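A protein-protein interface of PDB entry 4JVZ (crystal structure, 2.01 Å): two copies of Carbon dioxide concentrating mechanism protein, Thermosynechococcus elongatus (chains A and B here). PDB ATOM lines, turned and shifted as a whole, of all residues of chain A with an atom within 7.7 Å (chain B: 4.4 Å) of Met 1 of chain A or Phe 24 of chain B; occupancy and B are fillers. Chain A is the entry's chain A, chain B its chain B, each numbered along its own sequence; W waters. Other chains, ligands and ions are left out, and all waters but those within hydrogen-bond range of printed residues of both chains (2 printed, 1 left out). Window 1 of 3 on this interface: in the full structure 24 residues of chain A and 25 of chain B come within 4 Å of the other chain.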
ATOM      1  N   MET A   1       9.039   1.509  -8.178  1.00  0.00           N
ATOM      2  CA  MET A   1       9.736   1.018  -6.956  1.00  0.00           C
ATOM      3  C   MET A   1       8.788   1.045  -5.757  1.00  0.00           C
ATOM      4  O   MET A   1       7.802   1.782  -5.752  1.00  0.00           O
ATOM      5  CB  MET A   1      10.965   1.881  -6.657  1.00  0.00           C
ATOM      6  CG  MET A   1      12.074   1.793  -7.697  1.00  0.00           C
ATOM      7  SD  MET A   1      11.737   2.743  -9.190  1.00  0.00           S
ATOM      8  CE  MET A   1      12.368   4.357  -8.761  1.00  0.00           C
ATOM      9  N   LYS A   2       9.093   0.251  -4.735  1.00  0.00           N
ATOM     10  CA  LYS A   2       8.284   0.225  -3.521  1.00  0.00           C
ATOM     11  C   LYS A   2       9.104   0.665  -2.315  1.00  0.00           C
ATOM     12  O   LYS A   2      10.331   0.595  -2.321  1.00  0.00           O
ATOM     13  CB  LYS A   2       7.720  -1.178  -3.275  1.00  0.00           C
ATOM     14  CG  LYS A   2       6.801  -1.693  -4.366  1.00  0.00           C
ATOM     15  CD  LYS A   2       5.461  -0.972  -4.389  1.00  0.00           C
ATOM     16  CE  LYS A   2       4.484  -1.721  -5.283  1.00  0.00           C
ATOM     17  NZ  LYS A   2       3.422  -0.859  -5.873  1.00  0.00           N
ATOM     18  N   ILE A   3       8.406   1.125  -1.285  1.00  0.00           N
ATOM     19  CA  ILE A   3       9.028   1.523  -0.037  1.00  0.00           C
ATOM     20  C   ILE A   3       8.999   0.342   0.925  1.00  0.00           C
ATOM     21  O   ILE A   3       7.980  -0.336   1.056  1.00  0.00           O
ATOM     22  CB  ILE A   3       8.267   2.698   0.592  1.00  0.00           C
ATOM     23  CG1 ILE A   3       8.282   3.900  -0.355  1.00  0.00           C
ATOM     24  CG2 ILE A   3       8.876   3.067   1.937  1.00  0.00           C
ATOM     25  CD1 ILE A   3       7.430   5.064   0.111  1.00  0.00           C
ATOM     26  N   ALA A   4      10.110   0.096   1.608  1.00  0.00           N
ATOM     27  CA  ALA A   4      10.180  -1.010   2.552  1.00  0.00           C
ATOM     28  C   ALA A   4      11.109  -0.664   3.705  1.00  0.00           C
ATOM     29  O   ALA A   4      11.818   0.339   3.666  1.00  0.00           O
ATOM     30  CB  ALA A   4      10.651  -2.281   1.852  1.00  0.00           C
ATOM     31  N   TYR A  29       7.258  -4.653   3.261  1.00  0.00           N
ATOM     32  CA  TYR A  29       6.667  -3.584   2.462  1.00  0.00           C
ATOM     33  C   TYR A  29       5.782  -2.648   3.281  1.00  0.00           C
ATOM     34  O   TYR A  29       5.119  -3.064   4.226  1.00  0.00           O
ATOM     35  CB  TYR A  29       5.873  -4.168   1.293  1.00  0.00           C
ATOM     36  CG  TYR A  29       6.747  -4.681   0.170  1.00  0.00           C
ATOM     37  CD1 TYR A  29       7.523  -3.812  -0.578  1.00  0.00           C
ATOM     38  CD2 TYR A  29       6.797  -6.030  -0.140  1.00  0.00           C
ATOM     39  CE1 TYR A  29       8.323  -4.273  -1.598  1.00  0.00           C
ATOM     40  CE2 TYR A  29       7.593  -6.494  -1.158  1.00  0.00           C
ATOM     41  CZ  TYR A  29       8.354  -5.614  -1.885  1.00  0.00           C
ATOM     42  OH  TYR A  29       9.154  -6.078  -2.905  1.00  0.00           O
ATOM     43  N   VAL A  55      13.981   1.780   2.748  1.00  0.00           N
ATOM     44  CA  VAL A  55      14.643   1.627   1.460  1.00  0.00           C
ATOM     45  C   VAL A  55      13.658   1.658   0.299  1.00  0.00           C
ATOM     46  O   VAL A  55      12.464   1.408   0.470  1.00  0.00           O
ATOM     47  CB  VAL A  55      15.399   0.287   1.383  1.00  0.00           C
ATOM     48  CG1 VAL A  55      16.626   0.306   2.288  1.00  0.00           C
ATOM     49  CG2 VAL A  55      14.459  -0.874   1.729  1.00  0.00           C
ATOM     50  N   LEU A  56      14.172   1.967  -0.885  1.00  0.00           N
ATOM     51  CA  LEU A  56      13.431   1.757  -2.113  1.00  0.00           C
ATOM     52  C   LEU A  56      13.904   0.445  -2.716  1.00  0.00           C
ATOM     53  O   LEU A  56      15.104   0.217  -2.853  1.00  0.00           O
ATOM     54  CB  LEU A  56      13.676   2.897  -3.096  1.00  0.00           C
ATOM     55  CG  LEU A  56      13.190   4.270  -2.640  1.00  0.00           C
ATOM     56  CD1 LEU A  56      13.597   5.320  -3.665  1.00  0.00           C
ATOM     57  CD2 LEU A  56      11.675   4.251  -2.420  1.00  0.00           C
ATOM     58  N   VAL A  57      12.964  -0.421  -3.073  1.00  0.00           N
ATOM     59  CA  VAL A  57      13.309  -1.691  -3.695  1.00  0.00           C
ATOM     60  C   VAL A  57      12.827  -1.713  -5.133  1.00  0.00           C
ATOM     61  O   VAL A  57      11.675  -1.397  -5.412  1.00  0.00           O
ATOM     62  CB  VAL A  57      12.701  -2.906  -2.946  1.00  0.00           C
ATOM     63  CG1 VAL A  57      11.282  -2.600  -2.455  1.00  0.00           C
ATOM     64  CG2 VAL A  57      12.745  -4.150  -3.845  1.00  0.00           C
ATOM     65  N   SER A  58      13.718  -2.084  -6.043  1.00  0.00           N
ATOM     66  CA  SER A  58      13.358  -2.250  -7.439  1.00  0.00           C
ATOM     67  C   SER A  58      13.326  -3.744  -7.739  1.00  0.00           C
ATOM     68  O   SER A  58      14.187  -4.491  -7.281  1.00  0.00           O
ATOM     69  CB  SER A  58      14.369  -1.542  -8.341  1.00  0.00           C
ATOM     70  OG  SER A  58      14.430  -0.159  -8.042  1.00  0.00           O
ATOM     71  N   ARG A  59      12.331  -4.180  -8.500  1.00  0.00           N
ATOM     72  CA  ARG A  59      12.148  -5.598  -8.772  1.00  0.00           C
ATOM     73  C   ARG A  59      12.277  -5.883 -10.264  1.00  0.00           C
ATOM     74  O   ARG A  59      12.241  -4.967 -11.081  1.00  0.00           O
ATOM     75  CB  ARG A  59      10.773  -6.045  -8.281  1.00  0.00           C
ATOM     76  CG  ARG A  59      10.642  -6.133  -6.779  1.00  0.00           C
ATOM     77  CD  ARG A  59       9.185  -6.319  -6.413  1.00  0.00           C
ATOM     78  NE  ARG A  59       8.378  -5.195  -6.883  1.00  0.00           N
ATOM     79  CZ  ARG A  59       7.061  -5.229  -7.067  1.00  0.00           C
ATOM     80  NH1 ARG A  59       6.371  -6.336  -6.828  1.00  0.00           N
ATOM     81  NH2 ARG A  59       6.432  -4.146  -7.502  1.00  0.00           N
ATOM     82  N   ALA A  62      15.579  -4.769 -13.412  1.00  0.00           N
ATOM     83  CA  ALA A  62      16.218  -3.597 -12.826  1.00  0.00           C
ATOM     84  C   ALA A  62      17.287  -3.999 -11.817  1.00  0.00           C
ATOM     85  O   ALA A  62      18.352  -3.387 -11.751  1.00  0.00           O
ATOM     86  CB  ALA A  62      15.179  -2.728 -12.145  1.00  0.00           C
ATOM     87  N   ALA A  77      16.385  -5.746  -5.513  1.00  0.00           N
ATOM     88  CA  ALA A  77      17.537  -5.109  -4.906  1.00  0.00           C
ATOM     89  C   ALA A  77      17.148  -3.796  -4.249  1.00  0.00           C
ATOM     90  O   ALA A  77      16.302  -3.060  -4.750  1.00  0.00           O
ATOM     91  CB  ALA A  77      18.615  -4.868  -5.949  1.00  0.00           C
ATOM     92  N   VAL A  79      17.945  -0.182  -3.909  1.00  0.00           N
ATOM     93  CA  VAL A  79      18.634   0.738  -4.810  1.00  0.00           C
ATOM     94  C   VAL A  79      18.854   2.089  -4.157  1.00  0.00           C
ATOM     95  O   VAL A  79      19.577   2.933  -4.683  1.00  0.00           O
ATOM     96  CB  VAL A  79      17.869   0.939  -6.127  1.00  0.00           C
ATOM     97  CG1 VAL A  79      17.613  -0.404  -6.788  1.00  0.00           C
ATOM     98  CG2 VAL A  79      16.567   1.696  -5.884  1.00  0.00           C
ATOM     99  N   ALA A  80      18.242   2.286  -2.997  1.00  0.00           N
ATOM    100  CA  ALA A  80      18.403   3.533  -2.273  1.00  0.00           C
ATOM    101  C   ALA A  80      17.955   3.393  -0.827  1.00  0.00           C
ATOM    102  O   ALA A  80      17.033   2.642  -0.515  1.00  0.00           O
ATOM    103  CB  ALA A  80      17.627   4.648  -2.964  1.00  0.00           C
ATOM    104  N   SER A  86       7.867  12.547   1.483  1.00  0.00           N
ATOM    105  CA  SER A  86       6.851  13.563   1.679  1.00  0.00           C
ATOM    106  C   SER A  86       5.573  13.178   0.955  1.00  0.00           C
ATOM    107  O   SER A  86       5.611  12.777  -0.204  1.00  0.00           O
ATOM    108  CB  SER A  86       7.341  14.904   1.139  1.00  0.00           C
ATOM    109  OG  SER A  86       7.502  14.841  -0.268  1.00  0.00           O
ATOM    110  N   THR B   9       6.887  12.896  -2.578  1.00  0.00           N
ATOM    111  CA  THR B   9       8.260  12.751  -3.052  1.00  0.00           C
ATOM    112  C   THR B   9       9.115  11.876  -2.142  1.00  0.00           C
ATOM    113  O   THR B   9       8.851  11.755  -0.946  1.00  0.00           O
ATOM    114  CB  THR B   9       8.967  14.114  -3.147  1.00  0.00           C
ATOM    115  OG1 THR B   9       9.117  14.666  -1.833  1.00  0.00           O
ATOM    116  CG2 THR B   9       8.182  15.075  -4.018  1.00  0.00           C
ATOM    117  N   VAL B  10      10.159  11.291  -2.721  1.00  0.00           N
ATOM    118  CA  VAL B  10      11.156  10.544  -1.967  1.00  0.00           C
ATOM    119  C   VAL B  10      12.539  11.139  -2.227  1.00  0.00           C
ATOM    120  O   VAL B  10      12.875  11.450  -3.367  1.00  0.00           O
ATOM    121  CB  VAL B  10      11.171   9.059  -2.389  1.00  0.00           C
ATOM    122  CG1 VAL B  10      12.134   8.263  -1.504  1.00  0.00           C
ATOM    123  CG2 VAL B  10       9.761   8.476  -2.349  1.00  0.00           C
ATOM    124  N   VAL B  22      18.260  11.348 -10.370  1.00  0.00           N
ATOM    125  CA  VAL B  22      16.936  10.813 -10.669  1.00  0.00           C
ATOM    126  C   VAL B  22      15.922  11.289  -9.635  1.00  0.00           C
ATOM    127  O   VAL B  22      16.067  11.033  -8.441  1.00  0.00           O
ATOM    128  CB  VAL B  22      16.934   9.272 -10.721  1.00  0.00           C
ATOM    129  CG1 VAL B  22      15.513   8.746 -10.931  1.00  0.00           C
ATOM    130  CG2 VAL B  22      17.860   8.789 -11.827  1.00  0.00           C
ATOM    131  N   LYS B  23      14.898  11.989 -10.110  1.00  0.00           N
ATOM    132  CA  LYS B  23      13.836  12.497  -9.250  1.00  0.00           C
ATOM    133  C   LYS B  23      12.828  11.388  -8.978  1.00  0.00           C
ATOM    134  O   LYS B  23      12.413  10.694  -9.903  1.00  0.00           O
ATOM    135  CB  LYS B  23      13.130  13.674  -9.928  1.00  0.00           C
ATOM    136  CG  LYS B  23      11.809  14.042  -9.290  1.00  0.00           C
ATOM    137  CD  LYS B  23      11.804  15.474  -8.815  1.00  0.00           C
ATOM    138  CE  LYS B  23      10.658  15.718  -7.848  1.00  0.00           C
ATOM    139  NZ  LYS B  23      10.782  14.905  -6.600  1.00  0.00           N
ATOM    140  N   PHE B  24      12.426  11.229  -7.719  1.00  0.00           N
ATOM    141  CA  PHE B  24      11.492  10.174  -7.345  1.00  0.00           C
ATOM    142  C   PHE B  24      10.149  10.749  -6.913  1.00  0.00           C
ATOM    143  O   PHE B  24      10.082  11.615  -6.045  1.00  0.00           O
ATOM    144  CB  PHE B  24      12.075   9.322  -6.217  1.00  0.00           C
ATOM    145  CG  PHE B  24      13.370   8.666  -6.573  1.00  0.00           C
ATOM    146  CD1 PHE B  24      13.423   7.730  -7.582  1.00  0.00           C
ATOM    147  CD2 PHE B  24      14.534   8.990  -5.909  1.00  0.00           C
ATOM    148  CE1 PHE B  24      14.612   7.127  -7.922  1.00  0.00           C
ATOM    149  CE2 PHE B  24      15.724   8.388  -6.243  1.00  0.00           C
ATOM    150  CZ  PHE B  24      15.763   7.455  -7.251  1.00  0.00           C
ATOM    151  N   LEU B  25       9.080  10.257  -7.527  1.00  0.00           N
ATOM    152  CA  LEU B  25       7.743  10.688  -7.178  1.00  0.00           C
ATOM    153  C   LEU B  25       6.986   9.571  -6.488  1.00  0.00           C
ATOM    154  O   LEU B  25       7.090   8.405  -6.861  1.00  0.00           O
ATOM    155  CB  LEU B  25       6.984  11.127  -8.424  1.00  0.00           C
ATOM    156  CG  LEU B  25       7.533  12.392  -9.078  1.00  0.00           C
ATOM    157  CD1 LEU B  25       6.664  12.769 -10.264  1.00  0.00           C
ATOM    158  CD2 LEU B  25       7.619  13.528  -8.055  1.00  0.00           C
ATOM    159  N   VAL B  26       6.232   9.943  -5.465  1.00  0.00           N
ATOM    160  CA  VAL B  26       5.299   9.032  -4.836  1.00  0.00           C
ATOM    161  C   VAL B  26       3.991   9.127  -5.607  1.00  0.00           C
ATOM    162  O   VAL B  26       3.421  10.208  -5.736  1.00  0.00           O
ATOM    163  CB  VAL B  26       5.067   9.410  -3.368  1.00  0.00           C
ATOM    164  CG1 VAL B  26       4.011   8.503  -2.734  1.00  0.00           C
ATOM    165  CG2 VAL B  26       6.389   9.360  -2.606  1.00  0.00           C
ATOM    166  N   GLU B  41       3.099   3.823  -5.563  1.00  0.00           N
ATOM    167  CA  GLU B  41       4.279   3.405  -6.294  1.00  0.00           C
ATOM    168  C   GLU B  41       5.290   4.532  -6.211  1.00  0.00           C
ATOM    169  O   GLU B  41       4.923   5.697  -6.073  1.00  0.00           O
ATOM    170  CB  GLU B  41       3.949   3.104  -7.757  1.00  0.00           C
ATOM    171  CG  GLU B  41       5.111   2.487  -8.522  1.00  0.00           C
ATOM    172  CD  GLU B  41       5.182   0.978  -8.373  1.00  0.00           C
ATOM    173  OE1 GLU B  41       4.121   0.337  -8.215  1.00  0.00           O
ATOM    174  OE2 GLU B  41       6.304   0.428  -8.411  1.00  0.00           O
ATOM    175  N   VAL B  42       6.565   4.187  -6.289  1.00  0.00           N
ATOM    176  CA  VAL B  42       7.606   5.194  -6.335  1.00  0.00           C
ATOM    177  C   VAL B  42       8.248   5.115  -7.709  1.00  0.00           C
ATOM    178  O   VAL B  42       8.729   4.061  -8.119  1.00  0.00           O
ATOM    179  CB  VAL B  42       8.642   4.987  -5.225  1.00  0.00           C
ATOM    180  CG1 VAL B  42       9.674   6.113  -5.248  1.00  0.00           C
ATOM    181  CG2 VAL B  42       7.931   4.901  -3.876  1.00  0.00           C
ATOM    182  N   ALA B  43       8.234   6.228  -8.431  1.00  0.00           N
ATOM    183  CA  ALA B  43       8.621   6.209  -9.831  1.00  0.00           C
ATOM    184  C   ALA B  43       9.565   7.359 -10.166  1.00  0.00           C
ATOM    185  O   ALA B  43       9.523   8.418  -9.538  1.00  0.00           O
ATOM    186  CB  ALA B  43       7.381   6.256 -10.719  1.00  0.00           C
ATOM    187  N   ALA B  44      10.422   7.133 -11.154  1.00  0.00           N
ATOM    188  CA  ALA B  44      11.326   8.163 -11.635  1.00  0.00           C
ATOM    189  C   ALA B  44      10.552   9.113 -12.541  1.00  0.00           C
ATOM    190  O   ALA B  44       9.650   8.687 -13.263  1.00  0.00           O
ATOM    191  CB  ALA B  44      12.479   7.535 -12.389  1.00  0.00           C
ATOM    192  N   ILE B  74      15.822   1.055 -12.146  1.00  0.00           N
ATOM    193  CA  ILE B  74      14.499   1.568 -11.806  1.00  0.00           C
ATOM    194  C   ILE B  74      13.408   0.764 -12.509  1.00  0.00           C
ATOM    195  O   ILE B  74      13.492   0.500 -13.706  1.00  0.00           O
ATOM    196  CB  ILE B  74      14.366   3.057 -12.179  1.00  0.00           C
ATOM    197  CG1 ILE B  74      14.648   3.274 -13.671  1.00  0.00           C
ATOM    198  CG2 ILE B  74      15.333   3.877 -11.350  1.00  0.00           C
ATOM    199  CD1 ILE B  74      14.440   4.717 -14.149  1.00  0.00           C
ATOM    200  N   ASP B  75      12.385   0.371 -11.756  1.00  0.00           N
ATOM    201  CA  ASP B  75      11.322  -0.462 -12.299  1.00  0.00           C
ATOM    202  C   ASP B  75       9.989   0.276 -12.376  1.00  0.00           C
ATOM    203  O   ASP B  75       8.934  -0.350 -12.407  1.00  0.00           O
ATOM    204  CB  ASP B  75      11.163  -1.714 -11.440  1.00  0.00           C
ATOM    205  CG  ASP B  75      10.675  -1.396 -10.043  1.00  0.00           C
ATOM    206  OD1 ASP B  75      10.615  -0.199  -9.700  1.00  0.00           O
ATOM    207  OD2 ASP B  75      10.362  -2.341  -9.284  1.00  0.00           O
ATOM    208  N   ALA B  76      10.034   1.604 -12.400  1.00  0.00           N
ATOM    209  CA  ALA B  76       8.815   2.402 -12.512  1.00  0.00           C
ATOM    210  C   ALA B  76       9.136   3.837 -12.927  1.00  0.00           C
ATOM    211  O   ALA B  76      10.042   4.453 -12.374  1.00  0.00           O
ATOM    212  CB  ALA B  76       8.057   2.393 -11.194  1.00  0.00           C
HETATM  213  O   HOH W   1       9.314  -2.584  -6.704  1.00  0.00           O
HETATM  214  O   HOH W   2      10.528  13.842   0.486  1.00  0.00           O
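The backbone NH (N) of Met 1 of chain A is in hydrogen-bond range of the side-chain carboxylate (OE2) of Glu 41 of chain B (3.0 Å). N of Met 1 of chain A sits at hydrogen-bond distance from O of Val 42 of chain B (2.6 Å). The side-chain carboxylate (OD1) of Asp 75 of chain B is in hydrogen-bond range of the backbone NH (N) of Met 1 of chain A, 2.8 Å away. NZ of Lys 2 of chain A is in salt-bridge range of OE1 of Glu 41 of chain B, 2.7 Å away. The backbone NH of Arg 59 of chain A is in hydrogen-bond range of the side-chain carboxylate of Asp 75 of chain B (2.8 Å). The backbone carbonyl oxygen (O) of Ser 86 of chain A sits at hydrogen-bond distance from the backbone NH (N) of Thr 9 of chain B, 2.7 Å away.
The backbone carbonyl oxygen (O) of Lys 2 of chain A is in hydrogen-bond range of the backbone NH (N) of Val 57 of chain A (2.9 Å). The backbone carbonyl oxygen (O) of Leu 56 of chain A sits at hydrogen-bond distance from the backbone NH (N) of Val 79 of chain A. N of Leu 56 of chain A is in hydrogen-bond range of O of Ala 80 of chain A, 3.0 Å away. The backbone carbonyl oxygen of Ala 77 of chain A sits at hydrogen-bond distance from the backbone NH of Ser 58 of chain A, at 3.0 Å. The backbone NH (N) of Val 10 of chain B is in hydrogen-bond range of the backbone carbonyl oxygen (O) of Phe 24 of chain B (3.3 Å). N of Ala 44 of chain B sits at hydrogen-bond distance from O of Ala 76 of chain B (3.0 Å).
Among the printed residues, pairs that only touch across the chains: Met 1 of chain A with Ala 76 of chain B (3.3 Å), Ser 58 of chain A with Asp 75 of chain B (3.5 Å), Met 1 of chain A with Phe 24 of chain B (3.7 Å), Ile 3 of chain A with Val 42 of chain B (3.7 Å), Ala 62 of chain A with Ile 74 of chain B (3.8 Å), Leu 56 of chain A with Val 42 of chain B (3.9 Å), Leu 56 of chain A with Val 10 of chain B (3.9 Å) and Met 1 of chain A with Ile 74 of chain B (3.97 Å).
Met 1 of chain A touches just these residues of chain B: Phe 24 (3.7 Å), Glu 41 (3.0 Å), Val 42 (2.6 Å), Ile 74 (3.97 Å), Asp 75 (2.8 Å) and Ala 76 (3.3 Å). Phe 24 of chain B touches one residue of chain A. Printed residues of chain B within 4 Å of Ser 58 of chain A: Asp 75. Of the printed residues of chain A, Val 10 of chain B touches Leu 56. Of the printed residues of chain A, Thr 9 of chain B touches Ser 86 (2.3 Å). Of the printed residues of chain B, Ser 86 of chain A touches Thr 9 (2.3 Å). Of the printed residues of chain B, Ile 3 of chain A touches Val 42. Tyr 29 of chain A touches none of the printed residues of chain B. The nearest residue of chain B that does not touch Met 1 of chain A is Ala 44 of chain B (4.1 Å). The nearest printed residue of chain A that does not touch Thr 9 of chain B is Ile 3 of chain A (6.9 Å).
Hydrophobic or aromatic side chains of chain A within 4 Å of the printed part of chain B: Met 1, Ile 3, Leu 56 and Ala 62. Among the printed residues, Asp or Glu carboxylates within 4 Å of a Lys or Arg side-chain nitrogen of the other chain: Lys 2 of chain A with Glu 41 of chain B (2.7 Å).
No position is printed for both chains. Of the 14 pairs that touch across the chains among the printed residues, none has its exchanged pair printed and touching as well.
Water W1 lies within hydrogen-bond range of NE of Arg 59 of chain A (2.8 Å), OD2 of Asp 75 of chain B (2.8 Å), O of Val 57 of chain A (2.9 Å) and N of Lys 2 of chain A (3.5 Å). Water W2 lies within hydrogen-bond range of OG1 of Thr 9 of chain B (2.8 Å) and N of Ser 86 of chain A (3.1 Å).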
